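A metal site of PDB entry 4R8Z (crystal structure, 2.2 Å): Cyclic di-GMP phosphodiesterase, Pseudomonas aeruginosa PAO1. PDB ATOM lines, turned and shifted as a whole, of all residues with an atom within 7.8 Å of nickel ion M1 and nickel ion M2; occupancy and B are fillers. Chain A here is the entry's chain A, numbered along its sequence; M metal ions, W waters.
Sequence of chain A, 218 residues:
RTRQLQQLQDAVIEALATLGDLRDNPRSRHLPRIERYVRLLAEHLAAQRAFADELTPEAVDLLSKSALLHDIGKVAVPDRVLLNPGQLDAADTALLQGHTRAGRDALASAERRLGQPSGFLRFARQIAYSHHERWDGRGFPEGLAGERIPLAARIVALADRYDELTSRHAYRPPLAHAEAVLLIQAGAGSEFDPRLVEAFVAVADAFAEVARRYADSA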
ATOM      1  N   ASP A  21      25.464  24.638  -0.160  1.00  0.00           N
ATOM      2  CA  ASP A  21      26.133  25.699   0.637  1.00  0.00           C
ATOM      3  C   ASP A  21      26.620  26.815  -0.297  1.00  0.00           C
ATOM      4  O   ASP A  21      27.207  27.794   0.146  1.00  0.00           O
ATOM      5  CB  ASP A  21      27.351  25.102   1.357  1.00  0.00           C
ATOM      6  CG  ASP A  21      27.097  24.702   2.859  1.00  0.00           C
ATOM      7  OD1 ASP A  21      25.936  24.802   3.359  1.00  0.00           O
ATOM      8  OD2 ASP A  21      28.111  24.292   3.546  1.00  0.00           O
ATOM      9  N   ASP A  24      25.409  30.695   0.273  1.00  0.00           N
ATOM     10  CA  ASP A  24      25.825  31.494   1.412  1.00  0.00           C
ATOM     11  C   ASP A  24      27.150  31.110   2.013  1.00  0.00           C
ATOM     12  O   ASP A  24      27.560  31.771   2.947  1.00  0.00           O
ATOM     13  CB  ASP A  24      24.770  31.524   2.506  1.00  0.00           C
ATOM     14  CG  ASP A  24      24.728  30.221   3.300  1.00  0.00           C
ATOM     15  OD1 ASP A  24      25.087  29.153   2.756  1.00  0.00           O
ATOM     16  OD2 ASP A  24      24.316  30.266   4.473  1.00  0.00           O
ATOM     17  N   ASN A  25      27.825  30.070   1.515  1.00  0.00           N
ATOM     18  CA  ASN A  25      29.045  29.578   2.128  1.00  0.00           C
ATOM     19  C   ASN A  25      30.018  28.865   1.143  1.00  0.00           C
ATOM     20  O   ASN A  25      30.349  27.699   1.342  1.00  0.00           O
ATOM     21  CB  ASN A  25      28.674  28.653   3.294  1.00  0.00           C
ATOM     22  CG  ASN A  25      29.898  28.248   4.118  1.00  0.00           C
ATOM     23  OD1 ASN A  25      30.780  29.058   4.368  1.00  0.00           O
ATOM     24  ND2 ASN A  25      29.984  26.988   4.484  1.00  0.00           N
ATOM     25  N   HIS A  30      33.405  23.596   5.825  1.00  0.00           N
ATOM     26  CA  HIS A  30      32.391  23.428   6.861  1.00  0.00           C
ATOM     27  C   HIS A  30      31.900  21.977   7.008  1.00  0.00           C
ATOM     28  O   HIS A  30      31.789  21.463   8.107  1.00  0.00           O
ATOM     29  CB  HIS A  30      31.246  24.392   6.485  1.00  0.00           C
ATOM     30  CG  HIS A  30      29.994  24.312   7.295  1.00  0.00           C
ATOM     31  ND1 HIS A  30      29.987  24.434   8.661  1.00  0.00           N
ATOM     32  CD2 HIS A  30      28.677  24.181   6.923  1.00  0.00           C
ATOM     33  CE1 HIS A  30      28.726  24.385   9.109  1.00  0.00           C
ATOM     34  NE2 HIS A  30      27.905  24.255   8.066  1.00  0.00           N
ATOM     35  N   LEU A  31      31.608  21.327   5.904  1.00  0.00           N
ATOM     36  CA  LEU A  31      30.926  20.062   6.000  1.00  0.00           C
ATOM     37  C   LEU A  31      31.786  18.900   6.511  1.00  0.00           C
ATOM     38  O   LEU A  31      31.386  18.173   7.410  1.00  0.00           O
ATOM     39  CB  LEU A  31      30.272  19.667   4.681  1.00  0.00           C
ATOM     40  CG  LEU A  31      29.227  20.670   4.261  1.00  0.00           C
ATOM     41  CD1 LEU A  31      28.649  20.401   2.882  1.00  0.00           C
ATOM     42  CD2 LEU A  31      28.115  20.824   5.289  1.00  0.00           C
ATOM     43  N   ILE A  34      32.227  19.657  10.297  1.00  0.00           N
ATOM     44  CA  ILE A  34      31.053  19.366  11.116  1.00  0.00           C
ATOM     45  C   ILE A  34      30.895  17.891  11.350  1.00  0.00           C
ATOM     46  O   ILE A  34      30.631  17.417  12.474  1.00  0.00           O
ATOM     47  CB  ILE A  34      29.707  19.870  10.516  1.00  0.00           C
ATOM     48  CG1 ILE A  34      29.646  21.373  10.475  1.00  0.00           C
ATOM     49  CG2 ILE A  34      28.542  19.533  11.425  1.00  0.00           C
ATOM     50  CD1 ILE A  34      29.897  22.090  11.778  1.00  0.00           C
ATOM     51  N   ALA A  67      24.686  14.508   9.572  1.00  0.00           N
ATOM     52  CA  ALA A  67      24.886  15.917   9.955  1.00  0.00           C
ATOM     53  C   ALA A  67      25.235  16.797   8.783  1.00  0.00           C
ATOM     54  O   ALA A  67      24.951  17.975   8.801  1.00  0.00           O
ATOM     55  CB  ALA A  67      25.943  16.020  11.031  1.00  0.00           C
ATOM     56  N   LEU A  68      25.764  16.205   7.723  1.00  0.00           N
ATOM     57  CA  LEU A  68      26.060  16.955   6.502  1.00  0.00           C
ATOM     58  C   LEU A  68      24.852  17.681   5.867  1.00  0.00           C
ATOM     59  O   LEU A  68      25.032  18.687   5.134  1.00  0.00           O
ATOM     60  CB  LEU A  68      26.612  16.017   5.435  1.00  0.00           C
ATOM     61  CG  LEU A  68      27.970  15.379   5.648  1.00  0.00           C
ATOM     62  CD1 LEU A  68      28.334  14.472   4.461  1.00  0.00           C
ATOM     63  CD2 LEU A  68      29.043  16.401   5.749  1.00  0.00           C
ATOM     64  N   LEU A  69      23.663  17.168   6.106  1.00  0.00           N
ATOM     65  CA  LEU A  69      22.461  17.733   5.485  1.00  0.00           C
ATOM     66  C   LEU A  69      21.772  18.837   6.317  1.00  0.00           C
ATOM     67  O   LEU A  69      20.652  19.252   5.952  1.00  0.00           O
ATOM     68  CB  LEU A  69      21.468  16.593   5.207  1.00  0.00           C
ATOM     69  CG  LEU A  69      21.995  15.588   4.197  1.00  0.00           C
ATOM     70  CD1 LEU A  69      21.124  14.360   4.080  1.00  0.00           C
ATOM     71  CD2 LEU A  69      22.110  16.249   2.803  1.00  0.00           C
ATOM     72  N   HIS A  70      22.397  19.291   7.401  1.00  0.00           N
ATOM     73  CA  HIS A  70      21.704  20.169   8.367  1.00  0.00           C
ATOM     74  C   HIS A  70      21.093  21.351   7.671  1.00  0.00           C
ATOM     75  O   HIS A  70      19.970  21.737   8.002  1.00  0.00           O
ATOM     76  CB  HIS A  70      22.628  20.546   9.560  1.00  0.00           C
ATOM     77  CG  HIS A  70      23.791  21.429   9.224  1.00  0.00           C
ATOM     78  ND1 HIS A  70      24.974  20.937   8.692  1.00  0.00           N
ATOM     79  CD2 HIS A  70      23.951  22.772   9.306  1.00  0.00           C
ATOM     80  CE1 HIS A  70      25.797  21.946   8.458  1.00  0.00           C
ATOM     81  NE2 HIS A  70      25.167  23.074   8.765  1.00  0.00           N
ATOM     82  N   ASP A  71      21.769  21.940   6.715  1.00  0.00           N
ATOM     83  CA  ASP A  71      21.366  23.251   6.159  1.00  0.00           C
ATOM     84  C   ASP A  71      20.881  23.136   4.698  1.00  0.00           C
ATOM     85  O   ASP A  71      20.864  24.118   3.944  1.00  0.00           O
ATOM     86  CB  ASP A  71      22.569  24.272   6.195  1.00  0.00           C
ATOM     87  CG  ASP A  71      22.728  25.058   7.568  1.00  0.00           C
ATOM     88  OD1 ASP A  71      21.666  25.282   8.287  1.00  0.00           O
ATOM     89  OD2 ASP A  71      23.931  25.406   7.874  1.00  0.00           O
ATOM     90  N   ILE A  72      20.523  21.960   4.262  1.00  0.00           N
ATOM     91  CA  ILE A  72      20.095  21.858   2.818  1.00  0.00           C
ATOM     92  C   ILE A  72      18.817  22.624   2.494  1.00  0.00           C
ATOM     93  O   ILE A  72      18.575  22.971   1.354  1.00  0.00           O
ATOM     94  CB  ILE A  72      19.709  20.408   2.438  1.00  0.00           C
ATOM     95  CG1 ILE A  72      18.699  19.896   3.432  1.00  0.00           C
ATOM     96  CG2 ILE A  72      20.935  19.568   2.297  1.00  0.00           C
ATOM     97  CD1 ILE A  72      18.300  18.474   3.230  1.00  0.00           C
ATOM     98  N   LYS A  74      18.292  25.688   2.983  1.00  0.00           N
ATOM     99  CA  LYS A  74      18.519  27.094   2.697  1.00  0.00           C
ATOM    100  C   LYS A  74      18.089  27.581   1.340  1.00  0.00           C
ATOM    101  O   LYS A  74      18.006  28.787   1.145  1.00  0.00           O
ATOM    102  CB  LYS A  74      19.967  27.451   2.881  1.00  0.00           C
ATOM    103  CG  LYS A  74      20.202  27.823   4.344  1.00  0.00           C
ATOM    104  CD  LYS A  74      21.637  27.953   4.660  1.00  0.00           C
ATOM    105  CE  LYS A  74      21.788  28.393   6.122  1.00  0.00           C
ATOM    106  NZ  LYS A  74      23.248  28.203   6.458  1.00  0.00           N
ATOM    107  N   LEU A  96      14.545  33.212   7.043  1.00  0.00           N
ATOM    108  CA  LEU A  96      15.801  32.575   7.366  1.00  0.00           C
ATOM    109  C   LEU A  96      15.642  31.308   8.241  1.00  0.00           C
ATOM    110  O   LEU A  96      16.220  30.252   7.927  1.00  0.00           O
ATOM    111  CB  LEU A  96      16.716  33.592   8.028  1.00  0.00           C
ATOM    112  CG  LEU A  96      18.093  33.102   8.497  1.00  0.00           C
ATOM    113  CD1 LEU A  96      18.927  32.651   7.304  1.00  0.00           C
ATOM    114  CD2 LEU A  96      18.876  34.152   9.301  1.00  0.00           C
ATOM    115  N   GLN A  97      14.807  31.403   9.262  1.00  0.00           N
ATOM    116  CA  GLN A  97      14.473  30.278  10.115  1.00  0.00           C
ATOM    117  C   GLN A  97      13.806  29.107   9.395  1.00  0.00           C
ATOM    118  O   GLN A  97      14.000  27.918   9.774  1.00  0.00           O
ATOM    119  CB  GLN A  97      13.625  30.704  11.290  1.00  0.00           C
ATOM    120  CG  GLN A  97      14.387  31.694  12.191  1.00  0.00           C
ATOM    121  CD  GLN A  97      13.566  32.188  13.380  1.00  0.00           C
ATOM    122  OE1 GLN A  97      12.379  31.897  13.526  1.00  0.00           O
ATOM    123  NE2 GLN A  97      14.203  32.936  14.239  1.00  0.00           N
ATOM    124  N   HIS A  99      14.639  27.669   6.826  1.00  0.00           N
ATOM    125  CA  HIS A  99      15.570  26.621   6.342  1.00  0.00           C
ATOM    126  C   HIS A  99      15.390  25.283   7.052  1.00  0.00           C
ATOM    127  O   HIS A  99      15.576  24.239   6.452  1.00  0.00           O
ATOM    128  CB  HIS A  99      17.007  27.069   6.276  1.00  0.00           C
ATOM    129  CG  HIS A  99      17.785  26.956   7.563  1.00  0.00           C
ATOM    130  ND1 HIS A  99      17.720  27.900   8.559  1.00  0.00           N
ATOM    131  CD2 HIS A  99      18.759  26.097   7.932  1.00  0.00           C
ATOM    132  CE1 HIS A  99      18.588  27.583   9.519  1.00  0.00           C
ATOM    133  NE2 HIS A  99      19.274  26.533   9.137  1.00  0.00           N
ATOM    134  N   THR A 100      14.964  25.298   8.309  1.00  0.00           N
ATOM    135  CA  THR A 100      14.861  24.101   9.120  1.00  0.00           C
ATOM    136  C   THR A 100      13.641  23.320   8.630  1.00  0.00           C
ATOM    137  O   THR A 100      13.757  22.144   8.356  1.00  0.00           O
ATOM    138  CB  THR A 100      14.691  24.433  10.619  1.00  0.00           C
ATOM    139  OG1 THR A 100      13.643  25.408  10.773  1.00  0.00           O
ATOM    140  CG2 THR A 100      15.991  25.097  11.126  1.00  0.00           C
ATOM    141  N   ILE A 127      17.998  16.426  12.652  1.00  0.00           N
ATOM    142  CA  ILE A 127      19.003  17.446  12.622  1.00  0.00           C
ATOM    143  C   ILE A 127      18.559  18.625  11.805  1.00  0.00           C
ATOM    144  O   ILE A 127      18.711  19.782  12.197  1.00  0.00           O
ATOM    145  CB  ILE A 127      20.307  16.896  12.114  1.00  0.00           C
ATOM    146  CG1 ILE A 127      20.930  16.039  13.213  1.00  0.00           C
ATOM    147  CG2 ILE A 127      21.273  17.994  11.722  1.00  0.00           C
ATOM    148  CD1 ILE A 127      21.921  15.024  12.680  1.00  0.00           C
ATOM    149  N   ALA A 128      18.066  18.392  10.626  1.00  0.00           N
ATOM    150  CA  ALA A 128      17.758  19.552   9.808  1.00  0.00           C
ATOM    151  C   ALA A 128      16.726  20.431  10.487  1.00  0.00           C
ATOM    152  O   ALA A 128      16.734  21.653  10.363  1.00  0.00           O
ATOM    153  CB  ALA A 128      17.246  19.124   8.461  1.00  0.00           C
ATOM    154  N   HIS A 131      18.317  21.608  14.572  1.00  0.00           N
ATOM    155  CA  HIS A 131      19.698  22.018  14.831  1.00  0.00           C
ATOM    156  C   HIS A 131      19.890  23.485  15.387  1.00  0.00           C
ATOM    157  O   HIS A 131      20.968  23.826  15.832  1.00  0.00           O
ATOM    158  CB  HIS A 131      20.624  21.737  13.645  1.00  0.00           C
ATOM    159  CG  HIS A 131      20.527  22.656  12.472  1.00  0.00           C
ATOM    160  ND1 HIS A 131      19.577  22.535  11.483  1.00  0.00           N
ATOM    161  CD2 HIS A 131      21.299  23.694  12.094  1.00  0.00           C
ATOM    162  CE1 HIS A 131      19.734  23.479  10.582  1.00  0.00           C
ATOM    163  NE2 HIS A 131      20.756  24.239  10.949  1.00  0.00           N
ATOM    164  N   HIS A 132      18.847  24.308  15.360  1.00  0.00           N
ATOM    165  CA  HIS A 132      18.907  25.644  15.939  1.00  0.00           C
ATOM    166  C   HIS A 132      17.969  25.693  17.157  1.00  0.00           C
ATOM    167  O   HIS A 132      17.692  26.787  17.656  1.00  0.00           O
ATOM    168  CB  HIS A 132      18.502  26.699  14.951  1.00  0.00           C
ATOM    169  CG  HIS A 132      19.426  26.873  13.791  1.00  0.00           C
ATOM    170  ND1 HIS A 132      20.603  27.566  13.851  1.00  0.00           N
ATOM    171  CD2 HIS A 132      19.317  26.438  12.506  1.00  0.00           C
ATOM    172  CE1 HIS A 132      21.185  27.555  12.653  1.00  0.00           C
ATOM    173  NE2 HIS A 132      20.449  26.820  11.841  1.00  0.00           N
ATOM    174  N   PHE A 140      14.595  28.010  17.657  1.00  0.00           N
ATOM    175  CA  PHE A 140      13.587  27.876  16.652  1.00  0.00           C
ATOM    176  C   PHE A 140      13.797  26.555  15.902  1.00  0.00           C
ATOM    177  O   PHE A 140      14.907  26.034  15.945  1.00  0.00           O
ATOM    178  CB  PHE A 140      13.677  29.086  15.746  1.00  0.00           C
ATOM    179  CG  PHE A 140      14.973  29.240  14.972  1.00  0.00           C
ATOM    180  CD1 PHE A 140      15.172  28.590  13.757  1.00  0.00           C
ATOM    181  CD2 PHE A 140      15.972  30.126  15.439  1.00  0.00           C
ATOM    182  CE1 PHE A 140      16.353  28.733  13.031  1.00  0.00           C
ATOM    183  CE2 PHE A 140      17.141  30.347  14.700  1.00  0.00           C
ATOM    184  CZ  PHE A 140      17.332  29.624  13.485  1.00  0.00           C
ATOM    185  N   VAL A 156      24.646  18.394  17.123  1.00  0.00           N
ATOM    186  CA  VAL A 156      24.947  19.233  16.001  1.00  0.00           C
ATOM    187  C   VAL A 156      24.946  20.705  16.339  1.00  0.00           C
ATOM    188  O   VAL A 156      25.809  21.462  15.850  1.00  0.00           O
ATOM    189  CB  VAL A 156      24.036  18.958  14.795  1.00  0.00           C
ATOM    190  CG1 VAL A 156      24.275  19.927  13.647  1.00  0.00           C
ATOM    191  CG2 VAL A 156      24.292  17.583  14.293  1.00  0.00           C
ATOM    192  N   ASP A 160      28.078  22.965  15.392  1.00  0.00           N
ATOM    193  CA  ASP A 160      27.833  24.037  14.412  1.00  0.00           C
ATOM    194  C   ASP A 160      28.292  25.382  14.959  1.00  0.00           C
ATOM    195  O   ASP A 160      28.875  26.180  14.246  1.00  0.00           O
ATOM    196  CB  ASP A 160      26.353  24.078  14.127  1.00  0.00           C
ATOM    197  CG  ASP A 160      25.957  24.798  12.842  1.00  0.00           C
ATOM    198  OD1 ASP A 160      26.743  24.905  11.847  1.00  0.00           O
ATOM    199  OD2 ASP A 160      24.713  25.215  12.797  1.00  0.00           O
ATOM    200  N   ASP A 163      32.140  25.434  14.982  1.00  0.00           N
ATOM    201  CA  ASP A 163      32.620  25.671  13.644  1.00  0.00           C
ATOM    202  C   ASP A 163      32.444  27.103  13.161  1.00  0.00           C
ATOM    203  O   ASP A 163      33.343  27.680  12.540  1.00  0.00           O
ATOM    204  CB  ASP A 163      31.948  24.818  12.613  1.00  0.00           C
ATOM    205  CG  ASP A 163      32.748  24.810  11.280  1.00  0.00           C
ATOM    206  OD1 ASP A 163      33.972  24.451  11.324  1.00  0.00           O
ATOM    207  OD2 ASP A 163      32.203  25.196  10.238  1.00  0.00           O
HETATM  208 NI    NI M   1      25.874  24.737   7.820  1.00  0.00          NI
HETATM  209 NI    NI M   2      21.057  26.037  10.045  1.00  0.00          NI
HETATM  210  O   HOH W   1      21.776  27.661   9.353  1.00  0.00           O
HETATM  211  O   HOH W   2      26.088  25.670   9.597  1.00  0.00           O
HETATM  212  O   HOH W   3      25.772  23.833   5.983  1.00  0.00           O
HETATM  213  O   HOH W   4      23.037  25.904  10.591  1.00  0.00           O
HETATM  214  O   HOH W   5      26.329  26.432   6.880  1.00  0.00           O
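Nickel ion M1 is bound by water W5 (2.0 Å).
Nickel ion M1 is bound by water W2, 2.0 Å away.
Nickel ion M1 is bound by a ring nitrogen (NE2) of His 70 (2.0 Å).
Water W3 binds nickel ion M1, at 2.0 Å.
OD2 of Asp 71 is bound to nickel ion M1 (2.1 Å).
Nickel ion M1 is bound by a ring nitrogen (NE2) of His 30, at 2.1 Å.
Nickel ion M1 has six donor atoms within binding distance.
A ring nitrogen (ND1) of His 131 sits at hydrogen-bond distance from the backbone carbonyl oxygen of Ile 127 (3.0 Å).
The backbone carbonyl oxygen of His 132 is in hydrogen-bond range of the backbone NH of Phe 140.
A ring nitrogen (ND1) of His 131 lies within hydrogen-bond range of the backbone carbonyl oxygen (O) of Ala 128 (3.2 Å).
ND1 of His 70 is in hydrogen-bond range of O of Ala 67, at 3.0 Å.
O of Leu 96 lies within hydrogen-bond range of ND1 of His 99 (2.9 Å).
A ring nitrogen (ND1) of His 30 sits at hydrogen-bond distance from the side-chain carboxylate (OD2) of Asp 163 (2.8 Å).
The side-chain carboxylate (OD2) of Asp 71 lies close to the side-chain amino group (NZ) of Lys 74 (3.2 Å).
Of the 25 residues printed, 3 come within 4 Å of nickel ion M1.
The nearest printed residue that does not touch nickel ion M1 is Asp 160 (4.1 Å).
Four residues have an atom within 4 Å of nickel ion M2: Asp 71, His 99, His 131 and His 132.
Nickel ion M2 is bound by water W1 (1.9 Å), OD1 of Asp 71 (2.0 Å), NE2 of His 131 (2.0 Å), NE2 of His 132 (2.1 Å), water W4 (2.1 Å) and NE2 of His 99 (2.1 Å).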
